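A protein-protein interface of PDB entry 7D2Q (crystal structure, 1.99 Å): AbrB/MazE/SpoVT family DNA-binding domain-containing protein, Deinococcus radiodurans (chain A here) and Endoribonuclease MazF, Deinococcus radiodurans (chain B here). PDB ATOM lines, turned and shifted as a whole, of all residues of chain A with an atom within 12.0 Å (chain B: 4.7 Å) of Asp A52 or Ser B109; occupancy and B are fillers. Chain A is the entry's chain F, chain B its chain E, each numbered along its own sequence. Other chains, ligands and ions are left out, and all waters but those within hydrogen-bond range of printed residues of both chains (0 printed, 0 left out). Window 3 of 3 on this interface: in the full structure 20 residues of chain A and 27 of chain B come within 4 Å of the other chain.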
ATOM      1  N   TYR A  51     -13.655  15.767  -9.648  1.00  0.00           N
ATOM      2  CA  TYR A  51     -13.963  17.151 -10.029  1.00  0.00           C
ATOM      3  C   TYR A  51     -14.904  17.252 -11.216  1.00  0.00           C
ATOM      4  O   TYR A  51     -14.636  16.722 -12.291  1.00  0.00           O
ATOM      5  CB  TYR A  51     -12.682  17.925 -10.357  1.00  0.00           C
ATOM      6  CG  TYR A  51     -11.726  17.986  -9.203  1.00  0.00           C
ATOM      7  CD1 TYR A  51     -11.807  19.004  -8.270  1.00  0.00           C
ATOM      8  CD2 TYR A  51     -10.752  17.011  -9.038  1.00  0.00           C
ATOM      9  CE1 TYR A  51     -10.934  19.056  -7.201  1.00  0.00           C
ATOM     10  CE2 TYR A  51      -9.879  17.052  -7.973  1.00  0.00           C
ATOM     11  CZ  TYR A  51      -9.979  18.074  -7.062  1.00  0.00           C
ATOM     12  OH  TYR A  51      -9.111  18.117  -6.001  1.00  0.00           O
ATOM     13  N   ASP A  52     -16.000  17.970 -11.032  1.00  0.00           N
ATOM     14  CA  ASP A  52     -16.926  18.216 -12.121  1.00  0.00           C
ATOM     15  C   ASP A  52     -16.458  19.426 -12.926  1.00  0.00           C
ATOM     16  O   ASP A  52     -16.276  20.516 -12.371  1.00  0.00           O
ATOM     17  CB  ASP A  52     -18.334  18.428 -11.576  1.00  0.00           C
ATOM     18  CG  ASP A  52     -19.359  18.523 -12.667  1.00  0.00           C
ATOM     19  OD1 ASP A  52     -19.811  17.453 -13.150  1.00  0.00           O
ATOM     20  OD2 ASP A  52     -19.696  19.671 -13.039  1.00  0.00           O
ATOM     21  N   LEU A  53     -16.277  19.229 -14.236  1.00  0.00           N
ATOM     22  CA  LEU A  53     -15.648  20.254 -15.067  1.00  0.00           C
ATOM     23  C   LEU A  53     -16.485  21.529 -15.127  1.00  0.00           C
ATOM     24  O   LEU A  53     -15.944  22.636 -15.034  1.00  0.00           O
ATOM     25  CB  LEU A  53     -15.395  19.718 -16.477  1.00  0.00           C
ATOM     26  CG  LEU A  53     -14.737  20.748 -17.400  1.00  0.00           C
ATOM     27  CD1 LEU A  53     -13.434  21.245 -16.795  1.00  0.00           C
ATOM     28  CD2 LEU A  53     -14.495  20.183 -18.790  1.00  0.00           C
ATOM     29  N   ALA A  54     -17.805  21.402 -15.293  1.00  0.00           N
ATOM     30  CA  ALA A  54     -18.641  22.601 -15.318  1.00  0.00           C
ATOM     31  C   ALA A  54     -18.417  23.456 -14.077  1.00  0.00           C
ATOM     32  O   ALA A  54     -18.275  24.678 -14.178  1.00  0.00           O
ATOM     33  CB  ALA A  54     -20.116  22.221 -15.449  1.00  0.00           C
ATOM     34  N   ALA A  55     -18.347  22.826 -12.899  1.00  0.00           N
ATOM     35  CA  ALA A  55     -18.139  23.577 -11.662  1.00  0.00           C
ATOM     36  C   ALA A  55     -16.782  24.270 -11.649  1.00  0.00           C
ATOM     37  O   ALA A  55     -16.670  25.431 -11.230  1.00  0.00           O
ATOM     38  CB  ALA A  55     -18.269  22.651 -10.453  1.00  0.00           C
ATOM     39  N   LEU A  56     -15.733  23.574 -12.091  1.00  0.00           N
ATOM     40  CA  LEU A  56     -14.438  24.231 -12.247  1.00  0.00           C
ATOM     41  C   LEU A  56     -14.528  25.409 -13.210  1.00  0.00           C
ATOM     42  O   LEU A  56     -14.081  26.517 -12.891  1.00  0.00           O
ATOM     43  CB  LEU A  56     -13.394  23.222 -12.727  1.00  0.00           C
ATOM     44  CG  LEU A  56     -12.968  22.202 -11.688  1.00  0.00           C
ATOM     45  CD1 LEU A  56     -12.001  21.206 -12.325  1.00  0.00           C
ATOM     46  CD2 LEU A  56     -12.343  22.911 -10.499  1.00  0.00           C
ATOM     47  N   LEU A  57     -15.110  25.194 -14.400  1.00  0.00           N
ATOM     48  CA  LEU A  57     -15.084  26.246 -15.419  1.00  0.00           C
ATOM     49  C   LEU A  57     -15.862  27.481 -14.983  1.00  0.00           C
ATOM     50  O   LEU A  57     -15.506  28.607 -15.363  1.00  0.00           O
ATOM     51  CB  LEU A  57     -15.629  25.729 -16.750  1.00  0.00           C
ATOM     52  CG  LEU A  57     -14.826  24.608 -17.415  1.00  0.00           C
ATOM     53  CD1 LEU A  57     -15.291  24.378 -18.841  1.00  0.00           C
ATOM     54  CD2 LEU A  57     -13.336  24.922 -17.355  1.00  0.00           C
ATOM     55  N   ALA A  58     -16.921  27.293 -14.195  1.00  0.00           N
ATOM     56  CA  ALA A  58     -17.738  28.392 -13.700  1.00  0.00           C
ATOM     57  C   ALA A  58     -17.010  29.259 -12.682  1.00  0.00           C
ATOM     58  O   ALA A  58     -17.459  30.378 -12.412  1.00  0.00           O
ATOM     59  CB  ALA A  58     -19.026  27.843 -13.085  1.00  0.00           C
ATOM     60  N   GLU A  59     -15.898  28.783 -12.128  1.00  0.00           N
ATOM     61  CA  GLU A  59     -15.107  29.589 -11.216  1.00  0.00           C
ATOM     62  C   GLU A  59     -14.049  30.419 -11.932  1.00  0.00           C
ATOM     63  O   GLU A  59     -13.415  31.258 -11.292  1.00  0.00           O
ATOM     64  CB  GLU A  59     -14.435  28.693 -10.167  1.00  0.00           C
ATOM     65  CG  GLU A  59     -15.313  28.380  -8.966  1.00  0.00           C
ATOM     66  CD  GLU A  59     -15.055  26.997  -8.397  1.00  0.00           C
ATOM     67  OE1 GLU A  59     -13.937  26.463  -8.593  1.00  0.00           O
ATOM     68  OE2 GLU A  59     -15.971  26.447  -7.740  1.00  0.00           O
ATOM     69  N   MET A  60     -13.824  30.192 -13.226  1.00  0.00           N
ATOM     70  CA  MET A  60     -12.903  31.024 -13.989  1.00  0.00           C
ATOM     71  C   MET A  60     -13.556  32.360 -14.300  1.00  0.00           C
ATOM     72  O   MET A  60     -14.734  32.421 -14.658  1.00  0.00           O
ATOM     73  CB  MET A  60     -12.500  30.356 -15.302  1.00  0.00           C
ATOM     74  CG  MET A  60     -11.868  29.007 -15.165  1.00  0.00           C
ATOM     75  SD  MET A  60     -11.090  28.495 -16.704  1.00  0.00           S
ATOM     76  CE  MET A  60     -12.435  28.618 -17.878  1.00  0.00           C
ATOM     77  N   ARG B 104      -3.883  15.980 -10.844  1.00  0.00           N
ATOM     78  CA  ARG B 104      -4.343  15.016 -11.837  1.00  0.00           C
ATOM     79  C   ARG B 104      -5.858  15.036 -11.973  1.00  0.00           C
ATOM     80  O   ARG B 104      -6.388  14.923 -13.085  1.00  0.00           O
ATOM     81  CB  ARG B 104      -3.868  13.620 -11.463  1.00  0.00           C
ATOM     82  CG  ARG B 104      -2.372  13.465 -11.581  1.00  0.00           C
ATOM     83  CD  ARG B 104      -1.930  12.149 -10.989  1.00  0.00           C
ATOM     84  NE  ARG B 104      -0.567  11.841 -11.395  1.00  0.00           N
ATOM     85  CZ  ARG B 104       0.229  11.027 -10.722  1.00  0.00           C
ATOM     86  NH1 ARG B 104      -0.215  10.464  -9.608  1.00  0.00           N
ATOM     87  NH2 ARG B 104       1.458  10.778 -11.164  1.00  0.00           N
ATOM     88  N   GLY B 105      -6.570  15.168 -10.853  1.00  0.00           N
ATOM     89  CA  GLY B 105      -8.016  15.205 -10.921  1.00  0.00           C
ATOM     90  C   GLY B 105      -8.525  16.429 -11.654  1.00  0.00           C
ATOM     91  O   GLY B 105      -9.474  16.344 -12.437  1.00  0.00           O
ATOM     92  N   LYS B 106      -7.908  17.587 -11.409  1.00  0.00           N
ATOM     93  CA  LYS B 106      -8.374  18.796 -12.076  1.00  0.00           C
ATOM     94  C   LYS B 106      -8.003  18.774 -13.552  1.00  0.00           C
ATOM     95  O   LYS B 106      -8.833  19.081 -14.410  1.00  0.00           O
ATOM     96  CB  LYS B 106      -7.814  20.044 -11.381  1.00  0.00           C
ATOM     97  CG  LYS B 106      -8.493  20.312 -10.022  1.00  0.00           C
ATOM     98  CD  LYS B 106      -7.907  21.542  -9.338  1.00  0.00           C
ATOM     99  CE  LYS B 106      -8.622  21.839  -8.019  1.00  0.00           C
ATOM    100  NZ  LYS B 106      -8.130  23.106  -7.427  1.00  0.00           N
ATOM    101  N   LEU B 107      -6.764  18.410 -13.866  1.00  0.00           N
ATOM    102  CA  LEU B 107      -6.365  18.324 -15.268  1.00  0.00           C
ATOM    103  C   LEU B 107      -7.175  17.258 -15.994  1.00  0.00           C
ATOM    104  O   LEU B 107      -7.637  17.473 -17.121  1.00  0.00           O
ATOM    105  CB  LEU B 107      -4.861  18.037 -15.367  1.00  0.00           C
ATOM    106  CG  LEU B 107      -4.225  17.857 -16.752  1.00  0.00           C
ATOM    107  CD1 LEU B 107      -4.503  19.070 -17.639  1.00  0.00           C
ATOM    108  CD2 LEU B 107      -2.728  17.624 -16.592  1.00  0.00           C
ATOM    109  N   GLY B 108      -7.381  16.111 -15.349  1.00  0.00           N
ATOM    110  CA  GLY B 108      -8.161  15.057 -15.973  1.00  0.00           C
ATOM    111  C   GLY B 108      -9.569  15.503 -16.307  1.00  0.00           C
ATOM    112  O   GLY B 108     -10.112  15.147 -17.357  1.00  0.00           O
ATOM    113  N   SER B 109     -10.176  16.293 -15.417  1.00  0.00           N
ATOM    114  CA  SER B 109     -11.481  16.872 -15.700  1.00  0.00           C
ATOM    115  C   SER B 109     -11.432  17.732 -16.956  1.00  0.00           C
ATOM    116  O   SER B 109     -12.262  17.583 -17.860  1.00  0.00           O
ATOM    117  CB  SER B 109     -11.948  17.694 -14.497  1.00  0.00           C
ATOM    118  OG  SER B 109     -13.335  17.939 -14.585  1.00  0.00           O
ATOM    119  N   LEU B 110     -10.432  18.615 -17.043  1.00  0.00           N
ATOM    120  CA  LEU B 110     -10.299  19.496 -18.202  1.00  0.00           C
ATOM    121  C   LEU B 110     -10.097  18.705 -19.490  1.00  0.00           C
ATOM    122  O   LEU B 110     -10.676  19.037 -20.532  1.00  0.00           O
ATOM    123  CB  LEU B 110      -9.124  20.456 -17.994  1.00  0.00           C
ATOM    124  CG  LEU B 110      -8.816  21.358 -19.186  1.00  0.00           C
ATOM    125  CD1 LEU B 110     -10.027  22.260 -19.446  1.00  0.00           C
ATOM    126  CD2 LEU B 110      -7.554  22.170 -18.944  1.00  0.00           C
ATOM    127  N   LEU B 111      -9.274  17.659 -19.439  1.00  0.00           N
ATOM    128  CA  LEU B 111      -8.959  16.871 -20.622  1.00  0.00           C
ATOM    129  C   LEU B 111     -10.075  15.917 -21.020  1.00  0.00           C
ATOM    130  O   LEU B 111      -9.980  15.307 -22.089  1.00  0.00           O
ATOM    131  CB  LEU B 111      -7.665  16.081 -20.400  1.00  0.00           C
ATOM    132  CG  LEU B 111      -6.430  16.972 -20.292  1.00  0.00           C
ATOM    133  CD1 LEU B 111      -5.202  16.154 -19.966  1.00  0.00           C
ATOM    134  CD2 LEU B 111      -6.233  17.714 -21.594  1.00  0.00           C
ATOM    135  N   GLY B 112     -11.116  15.782 -20.203  1.00  0.00           N
ATOM    136  CA  GLY B 112     -12.233  14.918 -20.527  1.00  0.00           C
ATOM    137  C   GLY B 112     -12.048  13.466 -20.155  1.00  0.00           C
ATOM    138  O   GLY B 112     -12.684  12.596 -20.761  1.00  0.00           O
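Of the 10 printed residues of chain A, 3 touch a printed residue of chain B.
Hydrophobic or aromatic side chains of chain A within 4 Å of the printed part of chain B: Tyr A51 and Leu A53.
Among the printed residues, 6 pairs touch across the chains.
Among the printed residues, no Asp or Glu carboxylate lies within 4 Å of a Lys or Arg side-chain nitrogen of the other chain.
OG of Ser B109 sits at hydrogen-bond distance from O of Tyr A51 (2.9 Å).
The backbone NH of Leu A53 lies within hydrogen-bond range of the side-chain hydroxyl of Ser B109, 3.2 Å away.
The side-chain carboxylate of Asp A52 lies close to the backbone NH of Ala A54, 3.4 Å away.
The backbone NH (N) of Ala A55 sits at hydrogen-bond distance from the side-chain carboxylate (OD2) of Asp A52 (3.4 Å).
Printed residues of chain B within 4 Å of Tyr A51: Gly B105, Lys B106 and Ser B109.
Asp A52 touches just one residue of chain B: Ser B109 (3.8 Å).
Ala A55 touches none of the printed residues of chain B.
Of the printed residues of chain A, Gly B105 touches Tyr A51.
Printed residues of chain A within 4 Å of Lys B106: Tyr A51.
No residue of chain A comes within 4 Å of Leu B107.
No residue of chain A comes within 4 Å of Gly B108.
Ser B109 touches just these residues of chain A: Tyr A51 (2.9 Å), Asp A52 (3.8 Å) and Leu A53 (3.2 Å).
Leu B111 touches none of the printed residues of chain A.
No residue of chain A comes within 4 Å of Gly B112.
The nearest residue of chain A that does not touch Ser B109 is Leu A56 (4.1 Å).
The nearest printed residue of chain A that does not touch Lys B106 is Leu A56 (4.3 Å).
Among the printed residues, pairs that only touch across the chains: Tyr A51 with Gly B105, Tyr A51 with Lys B106, Asp A52 with Ser B109 and Leu A53 with Leu B110.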
